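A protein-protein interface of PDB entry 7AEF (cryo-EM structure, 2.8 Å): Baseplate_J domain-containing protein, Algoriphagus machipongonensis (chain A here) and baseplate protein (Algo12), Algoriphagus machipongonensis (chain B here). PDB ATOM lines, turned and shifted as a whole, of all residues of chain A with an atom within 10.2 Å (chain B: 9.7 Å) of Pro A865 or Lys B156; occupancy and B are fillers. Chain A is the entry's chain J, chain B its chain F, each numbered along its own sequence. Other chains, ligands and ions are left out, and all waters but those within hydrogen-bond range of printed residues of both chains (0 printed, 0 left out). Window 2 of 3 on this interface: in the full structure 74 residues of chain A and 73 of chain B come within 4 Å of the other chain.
Among the printed residues, merely in contact across the chains: Gly A866 with Lys B156 (3.996 Å), Phe A907 with Lys B120 (3.9 Å), Phe A907 with Arg B121 (3.2 Å), Phe A907 with Tyr B159 (3.6 Å), His A908 with Arg B121 (3.99 Å), His A908 with Gly B157 (3.7 Å), His A908 with Leu B158 (3.5 Å) and His A908 with Glu B192 (3.96 Å).
The side-chain amino group (NZ) of Lys B156 is in hydrogen-bond range of the backbone carbonyl oxygen (O) of Pro A865, at 3.3 Å. The backbone carbonyl oxygen (O) of Lys B156 is in hydrogen-bond range of a ring nitrogen (ND1) of His A908 (3.3 Å). OH of Tyr B159 sits close to NE2 of His A908 (3.3 Å). The side-chain carboxylate of Glu B192 is in hydrogen-bond range of the side-chain hydroxyl of Ser A906, 3.1 Å away.
Pro A865 touches just one residue of chain B: Lys B156. Of the printed residues of chain A, Lys B156 touches Pro A865 (3.3 Å), Gly A866 (3.996 Å) and His A908 (3.3 Å). Leu B155 touches none of the printed residues of chain A. Of chain A, only His A908 comes within 4 Å of Gly B157. Printed residues of chain B within 4 Å of Phe A907: Lys B120, Arg B121 and Tyr B159. Of the printed residues of chain B, Ser A906 touches Glu B192. Of the printed residues of chain A, Tyr B159 touches Phe A907 (3.6 Å) and His A908 (3.0 Å). Of the printed residues of chain A, Lys B120 touches Phe A907. Asn A867 touches none of the printed residues of chain B. Val B124 touches none of the printed residues of chain A.
NH1 of Arg B121 lies within hydrogen-bond range of O of Leu B155. The backbone NH (N) of Glu B122 sits at hydrogen-bond distance from the backbone carbonyl oxygen (O) of Leu B158, 2.9 Å away. O of Gly B157 lies within hydrogen-bond range of N of Asp B193. OH of Tyr B159 sits at hydrogen-bond distance from OE1 of Glu B192 (3.0 Å). N of Tyr B159 sits at hydrogen-bond distance from O of Asp B193 (2.8 Å). N of His A908 sits close to OG of Ser A906 (3.4 Å).
Of the 19 printed residues of chain A, 5 touch a printed residue of chain B. Printed residues of chain B that touch a printed residue of chain A: Lys B120, Arg B121, Lys B156, Gly B157, Leu B158, Tyr B159 and Glu B192. Hydrophobic or aromatic side chains of chain B within 4 Å of the printed part of chain A: Tyr B159. Along chain B the printed residues that touch a printed residue of chain A span positions 120 to 192. Among the printed residues, 12 pairs touch across the chains. Among the printed residues, no Asp or Glu carboxylate lies within 4 Å of a Lys or Arg side-chain nitrogen of the other chain.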
ATOM      1  N   LEU A 854       4.224  -0.616  15.328  1.00  0.00           N
ATOM      2  CA  LEU A 854       4.130  -1.765  14.424  1.00  0.00           C
ATOM      3  C   LEU A 854       3.386  -2.931  15.101  1.00  0.00           C
ATOM      4  O   LEU A 854       3.947  -3.640  15.944  1.00  0.00           O
ATOM      5  CB  LEU A 854       5.528  -2.178  13.957  1.00  0.00           C
ATOM      6  CG  LEU A 854       6.312  -1.228  13.039  1.00  0.00           C
ATOM      7  CD1 LEU A 854       7.088  -0.204  13.847  1.00  0.00           C
ATOM      8  CD2 LEU A 854       7.267  -2.000  12.160  1.00  0.00           C
ATOM      9  N   ASN A 855       2.158  -3.180  14.632  1.00  0.00           N
ATOM     10  CA  ASN A 855       1.149  -4.013  15.301  1.00  0.00           C
ATOM     11  C   ASN A 855       1.523  -5.481  15.532  1.00  0.00           C
ATOM     12  O   ASN A 855       1.086  -6.071  16.526  1.00  0.00           O
ATOM     13  CB  ASN A 855      -0.118  -3.983  14.485  1.00  0.00           C
ATOM     14  CG  ASN A 855      -0.857  -2.739  14.681  1.00  0.00           C
ATOM     15  OD1 ASN A 855      -0.716  -2.079  15.707  1.00  0.00           O
ATOM     16  ND2 ASN A 855      -1.665  -2.390  13.711  1.00  0.00           N
ATOM     17  N   HIS A 856       2.207  -6.129  14.595  1.00  0.00           N
ATOM     18  CA  HIS A 856       2.521  -7.546  14.781  1.00  0.00           C
ATOM     19  C   HIS A 856       4.009  -7.788  14.631  1.00  0.00           C
ATOM     20  O   HIS A 856       4.429  -8.883  14.256  1.00  0.00           O
ATOM     21  CB  HIS A 856       1.775  -8.436  13.792  1.00  0.00           C
ATOM     22  CG  HIS A 856       0.296  -8.397  13.934  1.00  0.00           C
ATOM     23  ND1 HIS A 856      -0.486  -7.474  13.278  1.00  0.00           N
ATOM     24  CD2 HIS A 856      -0.547  -9.179  14.642  1.00  0.00           C
ATOM     25  CE1 HIS A 856      -1.752  -7.680  13.591  1.00  0.00           C
ATOM     26  NE2 HIS A 856      -1.816  -8.711  14.416  1.00  0.00           N
ATOM     27  N   THR A 857       4.824  -6.775  14.900  1.00  0.00           N
ATOM     28  CA  THR A 857       6.232  -6.888  14.562  1.00  0.00           C
ATOM     29  C   THR A 857       7.092  -7.316  15.753  1.00  0.00           C
ATOM     30  O   THR A 857       7.079  -6.705  16.828  1.00  0.00           O
ATOM     31  CB  THR A 857       6.759  -5.575  14.004  1.00  0.00           C
ATOM     32  OG1 THR A 857       6.129  -5.357  12.741  1.00  0.00           O
ATOM     33  CG2 THR A 857       8.277  -5.666  13.740  1.00  0.00           C
ATOM     34  N   CYS A 858       7.836  -8.372  15.511  1.00  0.00           N
ATOM     35  CA  CYS A 858       8.960  -8.903  16.250  1.00  0.00           C
ATOM     36  C   CYS A 858      10.169  -8.881  15.354  1.00  0.00           C
ATOM     37  O   CYS A 858      10.016  -8.753  14.146  1.00  0.00           O
ATOM     38  CB  CYS A 858       8.655 -10.297  16.791  1.00  0.00           C
ATOM     39  SG  CYS A 858       7.024 -10.466  17.462  1.00  0.00           S
ATOM     40  N   SER A 861       9.629 -11.404  12.632  1.00  0.00           N
ATOM     41  CA  SER A 861       8.286 -11.644  12.120  1.00  0.00           C
ATOM     42  C   SER A 861       7.450 -10.380  11.977  1.00  0.00           C
ATOM     43  O   SER A 861       7.494  -9.490  12.826  1.00  0.00           O
ATOM     44  CB  SER A 861       7.543 -12.597  13.030  1.00  0.00           C
ATOM     45  OG  SER A 861       6.202 -12.747  12.611  1.00  0.00           O
ATOM     46  N   PHE A 862       6.632 -10.342  10.929  1.00  0.00           N
ATOM     47  CA  PHE A 862       5.671  -9.263  10.772  1.00  0.00           C
ATOM     48  C   PHE A 862       4.236  -9.758  10.906  1.00  0.00           C
ATOM     49  O   PHE A 862       3.305  -9.053  10.500  1.00  0.00           O
ATOM     50  CB  PHE A 862       5.899  -8.541   9.439  1.00  0.00           C
ATOM     51  CG  PHE A 862       7.199  -7.775   9.386  1.00  0.00           C
ATOM     52  CD1 PHE A 862       7.315  -6.562  10.024  1.00  0.00           C
ATOM     53  CD2 PHE A 862       8.301  -8.276   8.721  1.00  0.00           C
ATOM     54  CE1 PHE A 862       8.495  -5.855  10.004  1.00  0.00           C
ATOM     55  CE2 PHE A 862       9.487  -7.569   8.696  1.00  0.00           C
ATOM     56  CZ  PHE A 862       9.580  -6.358   9.339  1.00  0.00           C
ATOM     57  N   GLN A 863       4.051 -10.978  11.474  1.00  0.00           N
ATOM     58  CA  GLN A 863       2.739 -11.584  11.703  1.00  0.00           C
ATOM     59  C   GLN A 863       2.658 -12.336  13.045  1.00  0.00           C
ATOM     60  O   GLN A 863       1.978 -13.362  13.136  1.00  0.00           O
ATOM     61  CB  GLN A 863       2.381 -12.592  10.602  1.00  0.00           C
ATOM     62  CG  GLN A 863       2.109 -11.942   9.281  1.00  0.00           C
ATOM     63  CD  GLN A 863       0.804 -11.193   9.263  1.00  0.00           C
ATOM     64  OE1 GLN A 863      -0.265 -11.773   9.140  1.00  0.00           O
ATOM     65  NE2 GLN A 863       0.891  -9.875   9.442  1.00  0.00           N
ATOM     66  N   SER A 864       3.351 -11.874  14.090  1.00  0.00           N
ATOM     67  CA  SER A 864       3.255 -12.547  15.387  1.00  0.00           C
ATOM     68  C   SER A 864       2.317 -11.848  16.357  1.00  0.00           C
ATOM     69  O   SER A 864       2.547 -10.691  16.723  1.00  0.00           O
ATOM     70  CB  SER A 864       4.614 -12.746  16.036  1.00  0.00           C
ATOM     71  OG  SER A 864       5.499 -13.421  15.189  1.00  0.00           O
ATOM     72  N   PRO A 865       1.270 -12.540  16.794  1.00  0.00           N
ATOM     73  CA  PRO A 865       0.300 -11.960  17.724  1.00  0.00           C
ATOM     74  C   PRO A 865       0.895 -11.857  19.110  1.00  0.00           C
ATOM     75  O   PRO A 865       1.798 -12.610  19.467  1.00  0.00           O
ATOM     76  CB  PRO A 865      -0.851 -12.973  17.693  1.00  0.00           C
ATOM     77  CG  PRO A 865      -0.189 -14.266  17.338  1.00  0.00           C
ATOM     78  CD  PRO A 865       0.949 -13.926  16.433  1.00  0.00           C
ATOM     79  N   GLY A 866       0.384 -10.912  19.892  1.00  0.00           N
ATOM     80  CA  GLY A 866       0.813 -10.782  21.270  1.00  0.00           C
ATOM     81  C   GLY A 866       2.093 -10.011  21.477  1.00  0.00           C
ATOM     82  O   GLY A 866       2.775 -10.216  22.482  1.00  0.00           O
ATOM     83  N   ASN A 867       2.438  -9.112  20.568  1.00  0.00           N
ATOM     84  CA  ASN A 867       3.685  -8.372  20.681  1.00  0.00           C
ATOM     85  C   ASN A 867       3.538  -7.050  19.945  1.00  0.00           C
ATOM     86  O   ASN A 867       2.509  -6.801  19.313  1.00  0.00           O
ATOM     87  CB  ASN A 867       4.817  -9.215  20.119  1.00  0.00           C
ATOM     88  CG  ASN A 867       6.115  -8.968  20.796  1.00  0.00           C
ATOM     89  OD1 ASN A 867       6.448  -7.836  21.149  1.00  0.00           O
ATOM     90  ND2 ASN A 867       6.877 -10.024  20.978  1.00  0.00           N
ATOM     91  N   ALA A 868       4.578  -6.214  20.000  1.00  0.00           N
ATOM     92  CA  ALA A 868       4.593  -4.949  19.264  1.00  0.00           C
ATOM     93  C   ALA A 868       5.991  -4.354  19.250  1.00  0.00           C
ATOM     94  O   ALA A 868       6.745  -4.502  20.214  1.00  0.00           O
ATOM     95  CB  ALA A 868       3.638  -3.922  19.876  1.00  0.00           C
ATOM     96  N   THR A 869       6.302  -3.618  18.186  1.00  0.00           N
ATOM     97  CA  THR A 869       7.554  -2.870  18.112  1.00  0.00           C
ATOM     98  C   THR A 869       7.284  -1.390  17.863  1.00  0.00           C
ATOM     99  O   THR A 869       6.391  -1.017  17.098  1.00  0.00           O
ATOM    100  CB  THR A 869       8.515  -3.452  17.042  1.00  0.00           C
ATOM    101  OG1 THR A 869       8.847  -4.802  17.383  1.00  0.00           O
ATOM    102  CG2 THR A 869       9.805  -2.675  16.957  1.00  0.00           C
ATOM    103  N   SER A 906      -1.149  -3.924  29.114  1.00  0.00           N
ATOM    104  CA  SER A 906      -1.927  -5.070  29.507  1.00  0.00           C
ATOM    105  C   SER A 906      -1.009  -5.964  30.271  1.00  0.00           C
ATOM    106  O   SER A 906       0.188  -6.003  29.971  1.00  0.00           O
ATOM    107  CB  SER A 906      -2.488  -5.842  28.324  1.00  0.00           C
ATOM    108  OG  SER A 906      -3.127  -7.010  28.791  1.00  0.00           O
ATOM    109  N   PHE A 907      -1.584  -6.726  31.193  1.00  0.00           N
ATOM    110  CA  PHE A 907      -0.815  -7.722  31.915  1.00  0.00           C
ATOM    111  C   PHE A 907      -0.026  -8.647  30.984  1.00  0.00           C
ATOM    112  O   PHE A 907       1.113  -9.016  31.286  1.00  0.00           O
ATOM    113  CB  PHE A 907      -1.745  -8.547  32.786  1.00  0.00           C
ATOM    114  CG  PHE A 907      -1.041  -9.623  33.481  1.00  0.00           C
ATOM    115  CD1 PHE A 907      -0.233  -9.337  34.552  1.00  0.00           C
ATOM    116  CD2 PHE A 907      -1.132 -10.920  33.036  1.00  0.00           C
ATOM    117  CE1 PHE A 907       0.453 -10.333  35.176  1.00  0.00           C
ATOM    118  CE2 PHE A 907      -0.447 -11.909  33.647  1.00  0.00           C
ATOM    119  CZ  PHE A 907       0.344 -11.623  34.721  1.00  0.00           C
ATOM    120  N   HIS A 908      -0.587  -8.969  29.826  1.00  0.00           N
ATOM    121  CA  HIS A 908      -0.011  -9.947  28.925  1.00  0.00           C
ATOM    122  C   HIS A 908       0.921  -9.400  27.844  1.00  0.00           C
ATOM    123  O   HIS A 908       1.360 -10.193  27.007  1.00  0.00           O
ATOM    124  CB  HIS A 908      -1.130 -10.696  28.222  1.00  0.00           C
ATOM    125  CG  HIS A 908      -2.009 -11.465  29.143  1.00  0.00           C
ATOM    126  ND1 HIS A 908      -1.623 -12.656  29.715  1.00  0.00           N
ATOM    127  CD2 HIS A 908      -3.264 -11.223  29.583  1.00  0.00           C
ATOM    128  CE1 HIS A 908      -2.603 -13.113  30.471  1.00  0.00           C
ATOM    129  NE2 HIS A 908      -3.610 -12.261  30.409  1.00  0.00           N
ATOM    130  N   VAL A 909       1.199  -8.094  27.739  1.00  0.00           N
ATOM    131  CA  VAL A 909       1.955  -7.617  26.569  1.00  0.00           C
ATOM    132  C   VAL A 909       3.138  -6.708  26.913  1.00  0.00           C
ATOM    133  O   VAL A 909       2.988  -5.683  27.589  1.00  0.00           O
ATOM    134  CB  VAL A 909       1.048  -6.912  25.543  1.00  0.00           C
ATOM    135  CG1 VAL A 909       1.878  -6.361  24.358  1.00  0.00           C
ATOM    136  CG2 VAL A 909       0.014  -7.876  25.004  1.00  0.00           C
ATOM    137  N   GLN A 910       4.303  -7.058  26.372  1.00  0.00           N
ATOM    138  CA  GLN A 910       5.485  -6.219  26.429  1.00  0.00           C
ATOM    139  C   GLN A 910       5.826  -5.708  25.041  1.00  0.00           C
ATOM    140  O   GLN A 910       5.780  -6.463  24.071  1.00  0.00           O
ATOM    141  CB  GLN A 910       6.687  -6.975  27.000  1.00  0.00           C
ATOM    142  CG  GLN A 910       6.397  -7.531  28.356  1.00  0.00           C
ATOM    143  CD  GLN A 910       6.583  -6.481  29.432  1.00  0.00           C
ATOM    144  OE1 GLN A 910       7.584  -5.764  29.476  1.00  0.00           O
ATOM    145  NE2 GLN A 910       5.536  -6.295  30.228  1.00  0.00           N
ATOM    146  N   LYS B 120      -2.186 -13.176  38.116  1.00  0.00           N
ATOM    147  CA  LYS B 120      -1.173 -14.001  37.489  1.00  0.00           C
ATOM    148  C   LYS B 120      -1.728 -14.559  36.191  1.00  0.00           C
ATOM    149  O   LYS B 120      -2.945 -14.614  36.002  1.00  0.00           O
ATOM    150  CB  LYS B 120      -0.742 -15.133  38.426  1.00  0.00           C
ATOM    151  CG  LYS B 120      -0.221 -14.672  39.803  1.00  0.00           C
ATOM    152  CD  LYS B 120       1.084 -13.874  39.705  1.00  0.00           C
ATOM    153  CE  LYS B 120       1.654 -13.531  41.084  1.00  0.00           C
ATOM    154  NZ  LYS B 120       2.865 -12.638  40.999  1.00  0.00           N
ATOM    155  N   ARG B 121      -0.819 -15.027  35.333  1.00  0.00           N
ATOM    156  CA  ARG B 121      -1.111 -15.518  33.983  1.00  0.00           C
ATOM    157  C   ARG B 121      -1.027 -17.036  33.909  1.00  0.00           C
ATOM    158  O   ARG B 121      -0.029 -17.607  34.362  1.00  0.00           O
ATOM    159  CB  ARG B 121      -0.078 -14.975  33.004  1.00  0.00           C
ATOM    160  CG  ARG B 121       0.059 -15.800  31.734  1.00  0.00           C
ATOM    161  CD  ARG B 121       1.347 -15.547  31.006  1.00  0.00           C
ATOM    162  NE  ARG B 121       1.295 -16.163  29.690  1.00  0.00           N
ATOM    163  CZ  ARG B 121       2.317 -16.226  28.854  1.00  0.00           C
ATOM    164  NH1 ARG B 121       2.173 -16.812  27.677  1.00  0.00           N
ATOM    165  NH2 ARG B 121       3.480 -15.704  29.195  1.00  0.00           N
ATOM    166  N   GLU B 122      -2.033 -17.676  33.299  1.00  0.00           N
ATOM    167  CA  GLU B 122      -1.993 -19.109  33.073  1.00  0.00           C
ATOM    168  C   GLU B 122      -1.177 -19.484  31.859  1.00  0.00           C
ATOM    169  O   GLU B 122      -1.190 -18.784  30.849  1.00  0.00           O
ATOM    170  CB  GLU B 122      -3.379 -19.682  32.879  1.00  0.00           C
ATOM    171  CG  GLU B 122      -4.274 -19.532  34.020  1.00  0.00           C
ATOM    172  CD  GLU B 122      -3.781 -20.417  35.075  1.00  0.00           C
ATOM    173  OE1 GLU B 122      -3.988 -21.618  35.007  1.00  0.00           O
ATOM    174  OE2 GLU B 122      -3.222 -19.901  36.025  1.00  0.00           O
ATOM    175  N   ARG B 123      -0.501 -20.628  31.948  1.00  0.00           N
ATOM    176  CA  ARG B 123       0.261 -21.167  30.816  1.00  0.00           C
ATOM    177  C   ARG B 123      -0.319 -22.536  30.481  1.00  0.00           C
ATOM    178  O   ARG B 123       0.100 -23.541  31.062  1.00  0.00           O
ATOM    179  CB  ARG B 123       1.760 -21.251  31.126  1.00  0.00           C
ATOM    180  CG  ARG B 123       2.402 -19.912  31.455  1.00  0.00           C
ATOM    181  CD  ARG B 123       3.889 -20.039  31.728  1.00  0.00           C
ATOM    182  NE  ARG B 123       4.526 -18.746  31.950  1.00  0.00           N
ATOM    183  CZ  ARG B 123       4.663 -18.199  33.162  1.00  0.00           C
ATOM    184  NH1 ARG B 123       4.217 -18.833  34.236  1.00  0.00           N
ATOM    185  NH2 ARG B 123       5.251 -17.022  33.294  1.00  0.00           N
ATOM    186  N   VAL B 124      -1.301 -22.553  29.583  1.00  0.00           N
ATOM    187  CA  VAL B 124      -1.917 -23.780  29.127  1.00  0.00           C
ATOM    188  C   VAL B 124      -1.073 -24.263  27.975  1.00  0.00           C
ATOM    189  O   VAL B 124      -0.711 -23.480  27.100  1.00  0.00           O
ATOM    190  CB  VAL B 124      -3.364 -23.525  28.702  1.00  0.00           C
ATOM    191  CG1 VAL B 124      -3.991 -24.781  28.145  1.00  0.00           C
ATOM    192  CG2 VAL B 124      -4.135 -22.998  29.889  1.00  0.00           C
ATOM    193  N   THR B 125      -0.687 -25.515  27.996  1.00  0.00           N
ATOM    194  CA  THR B 125       0.163 -26.041  26.947  1.00  0.00           C
ATOM    195  C   THR B 125      -0.545 -26.961  25.995  1.00  0.00           C
ATOM    196  O   THR B 125      -1.257 -27.876  26.409  1.00  0.00           O
ATOM    197  CB  THR B 125       1.349 -26.744  27.557  1.00  0.00           C
ATOM    198  OG1 THR B 125       0.861 -27.887  28.268  1.00  0.00           O
ATOM    199  CG2 THR B 125       2.140 -25.846  28.425  1.00  0.00           C
ATOM    200  N   VAL B 126      -0.244 -26.752  24.723  1.00  0.00           N
ATOM    201  CA  VAL B 126      -0.757 -27.553  23.631  1.00  0.00           C
ATOM    202  C   VAL B 126       0.408 -28.181  22.893  1.00  0.00           C
ATOM    203  O   VAL B 126       1.385 -27.506  22.549  1.00  0.00           O
ATOM    204  CB  VAL B 126      -1.624 -26.702  22.697  1.00  0.00           C
ATOM    205  CG1 VAL B 126      -2.062 -27.506  21.494  1.00  0.00           C
ATOM    206  CG2 VAL B 126      -2.840 -26.241  23.465  1.00  0.00           C
ATOM    207  N   PHE B 153       3.040 -25.195  21.968  1.00  0.00           N
ATOM    208  CA  PHE B 153       2.805 -23.760  22.051  1.00  0.00           C
ATOM    209  C   PHE B 153       2.026 -23.501  23.331  1.00  0.00           C
ATOM    210  O   PHE B 153       1.326 -24.385  23.836  1.00  0.00           O
ATOM    211  CB  PHE B 153       2.187 -23.187  20.743  1.00  0.00           C
ATOM    212  CG  PHE B 153       0.763 -23.576  20.488  1.00  0.00           C
ATOM    213  CD1 PHE B 153      -0.274 -22.923  21.131  1.00  0.00           C
ATOM    214  CD2 PHE B 153       0.456 -24.574  19.584  1.00  0.00           C
ATOM    215  CE1 PHE B 153      -1.583 -23.272  20.899  1.00  0.00           C
ATOM    216  CE2 PHE B 153      -0.861 -24.925  19.347  1.00  0.00           C
ATOM    217  CZ  PHE B 153      -1.878 -24.271  20.004  1.00  0.00           C
ATOM    218  N   ASP B 154       2.237 -22.322  23.897  1.00  0.00           N
ATOM    219  CA  ASP B 154       1.601 -21.904  25.136  1.00  0.00           C
ATOM    220  C   ASP B 154       0.521 -20.891  24.834  1.00  0.00           C
ATOM    221  O   ASP B 154       0.657 -20.113  23.896  1.00  0.00           O
ATOM    222  CB  ASP B 154       2.614 -21.339  26.139  1.00  0.00           C
ATOM    223  CG  ASP B 154       3.713 -22.331  26.502  1.00  0.00           C
ATOM    224  OD1 ASP B 154       3.555 -23.526  26.241  1.00  0.00           O
ATOM    225  OD2 ASP B 154       4.702 -21.922  27.098  1.00  0.00           O
ATOM    226  N   LEU B 155      -0.534 -20.861  25.637  1.00  0.00           N
ATOM    227  CA  LEU B 155      -1.592 -19.892  25.365  1.00  0.00           C
ATOM    228  C   LEU B 155      -1.253 -18.501  25.933  1.00  0.00           C
ATOM    229  O   LEU B 155      -0.609 -18.362  26.978  1.00  0.00           O
ATOM    230  CB  LEU B 155      -2.943 -20.412  25.877  1.00  0.00           C
ATOM    231  CG  LEU B 155      -3.725 -21.358  24.904  1.00  0.00           C
ATOM    232  CD1 LEU B 155      -2.990 -22.688  24.653  1.00  0.00           C
ATOM    233  CD2 LEU B 155      -5.106 -21.644  25.459  1.00  0.00           C
ATOM    234  N   LYS B 156      -1.722 -17.444  25.234  1.00  0.00           N
ATOM    235  CA  LYS B 156      -1.297 -16.059  25.521  1.00  0.00           C
ATOM    236  C   LYS B 156      -2.256 -15.126  26.299  1.00  0.00           C
ATOM    237  O   LYS B 156      -1.775 -14.079  26.743  1.00  0.00           O
ATOM    238  CB  LYS B 156      -0.907 -15.339  24.223  1.00  0.00           C
ATOM    239  CG  LYS B 156       0.354 -15.874  23.561  1.00  0.00           C
ATOM    240  CD  LYS B 156       1.111 -14.807  22.806  1.00  0.00           C
ATOM    241  CE  LYS B 156       2.485 -15.275  22.372  1.00  0.00           C
ATOM    242  NZ  LYS B 156       3.326 -14.136  21.933  1.00  0.00           N
ATOM    243  N   GLY B 157      -3.550 -15.426  26.506  1.00  0.00           N
ATOM    244  CA  GLY B 157      -4.384 -14.448  27.230  1.00  0.00           C
ATOM    245  C   GLY B 157      -5.239 -14.929  28.401  1.00  0.00           C
ATOM    246  O   GLY B 157      -6.368 -14.459  28.576  1.00  0.00           O
ATOM    247  N   LEU B 158      -4.756 -15.852  29.220  1.00  0.00           N
ATOM    248  CA  LEU B 158      -5.593 -16.389  30.285  1.00  0.00           C
ATOM    249  C   LEU B 158      -5.141 -15.999  31.699  1.00  0.00           C
ATOM    250  O   LEU B 158      -3.942 -15.975  31.990  1.00  0.00           O
ATOM    251  CB  LEU B 158      -5.640 -17.896  30.119  1.00  0.00           C
ATOM    252  CG  LEU B 158      -6.143 -18.391  28.748  1.00  0.00           C
ATOM    253  CD1 LEU B 158      -6.054 -19.895  28.730  1.00  0.00           C
ATOM    254  CD2 LEU B 158      -7.571 -17.908  28.471  1.00  0.00           C
ATOM    255  N   TYR B 159      -6.114 -15.758  32.603  1.00  0.00           N
ATOM    256  CA  TYR B 159      -5.857 -15.318  33.984  1.00  0.00           C
ATOM    257  C   TYR B 159      -6.218 -16.270  35.139  1.00  0.00           C
ATOM    258  O   TYR B 159      -7.181 -17.050  35.085  1.00  0.00           O
ATOM    259  CB  TYR B 159      -6.618 -14.034  34.299  1.00  0.00           C
ATOM    260  CG  TYR B 159      -6.221 -12.841  33.541  1.00  0.00           C
ATOM    261  CD1 TYR B 159      -6.965 -12.411  32.470  1.00  0.00           C
ATOM    262  CD2 TYR B 159      -5.106 -12.142  33.905  1.00  0.00           C
ATOM    263  CE1 TYR B 159      -6.597 -11.295  31.780  1.00  0.00           C
ATOM    264  CE2 TYR B 159      -4.726 -11.026  33.233  1.00  0.00           C
ATOM    265  CZ  TYR B 159      -5.468 -10.600  32.164  1.00  0.00           C
ATOM    266  OH  TYR B 159      -5.084  -9.471  31.474  1.00  0.00           O
ATOM    267  N   LEU B 190     -10.537  -7.297  25.074  1.00  0.00           N
ATOM    268  CA  LEU B 190     -10.733  -8.148  23.909  1.00  0.00           C
ATOM    269  C   LEU B 190      -9.651  -9.225  23.850  1.00  0.00           C
ATOM    270  O   LEU B 190      -8.467  -8.916  24.007  1.00  0.00           O
ATOM    271  CB  LEU B 190     -10.704  -7.278  22.646  1.00  0.00           C
ATOM    272  CG  LEU B 190     -11.031  -7.922  21.293  1.00  0.00           C
ATOM    273  CD1 LEU B 190     -12.480  -8.346  21.246  1.00  0.00           C
ATOM    274  CD2 LEU B 190     -10.736  -6.945  20.185  1.00  0.00           C
ATOM    275  N   CYS B 191     -10.070 -10.481  23.612  1.00  0.00           N
ATOM    276  CA  CYS B 191      -9.210 -11.680  23.480  1.00  0.00           C
ATOM    277  C   CYS B 191      -8.495 -12.110  24.761  1.00  0.00           C
ATOM    278  O   CYS B 191      -7.359 -12.590  24.705  1.00  0.00           O
ATOM    279  CB  CYS B 191      -8.166 -11.515  22.384  1.00  0.00           C
ATOM    280  SG  CYS B 191      -8.867 -11.236  20.798  1.00  0.00           S
ATOM    281  N   GLU B 192      -9.171 -11.987  25.909  1.00  0.00           N
ATOM    282  CA  GLU B 192      -8.627 -12.405  27.205  1.00  0.00           C
ATOM    283  C   GLU B 192      -9.723 -13.089  28.029  1.00  0.00           C
ATOM    284  O   GLU B 192     -10.907 -12.778  27.871  1.00  0.00           O
ATOM    285  CB  GLU B 192      -8.081 -11.188  27.956  1.00  0.00           C
ATOM    286  CG  GLU B 192      -6.939 -10.471  27.245  1.00  0.00           C
ATOM    287  CD  GLU B 192      -6.390  -9.309  28.036  1.00  0.00           C
ATOM    288  OE1 GLU B 192      -6.908  -9.047  29.141  1.00  0.00           O
ATOM    289  OE2 GLU B 192      -5.464  -8.637  27.539  1.00  0.00           O
ATOM    290  N   ASP B 193      -9.335 -14.020  28.917  1.00  0.00           N
ATOM    291  CA  ASP B 193     -10.331 -14.716  29.743  1.00  0.00           C
ATOM    292  C   ASP B 193      -9.791 -15.150  31.109  1.00  0.00           C
ATOM    293  O   ASP B 193      -8.585 -15.259  31.325  1.00  0.00           O
ATOM    294  CB  ASP B 193     -10.893 -15.935  29.002  1.00  0.00           C
ATOM    295  CG  ASP B 193     -12.235 -16.391  29.552  1.00  0.00           C
ATOM    296  OD1 ASP B 193     -12.768 -15.703  30.420  1.00  0.00           O
ATOM    297  OD2 ASP B 193     -12.767 -17.399  29.099  1.00  0.00           O
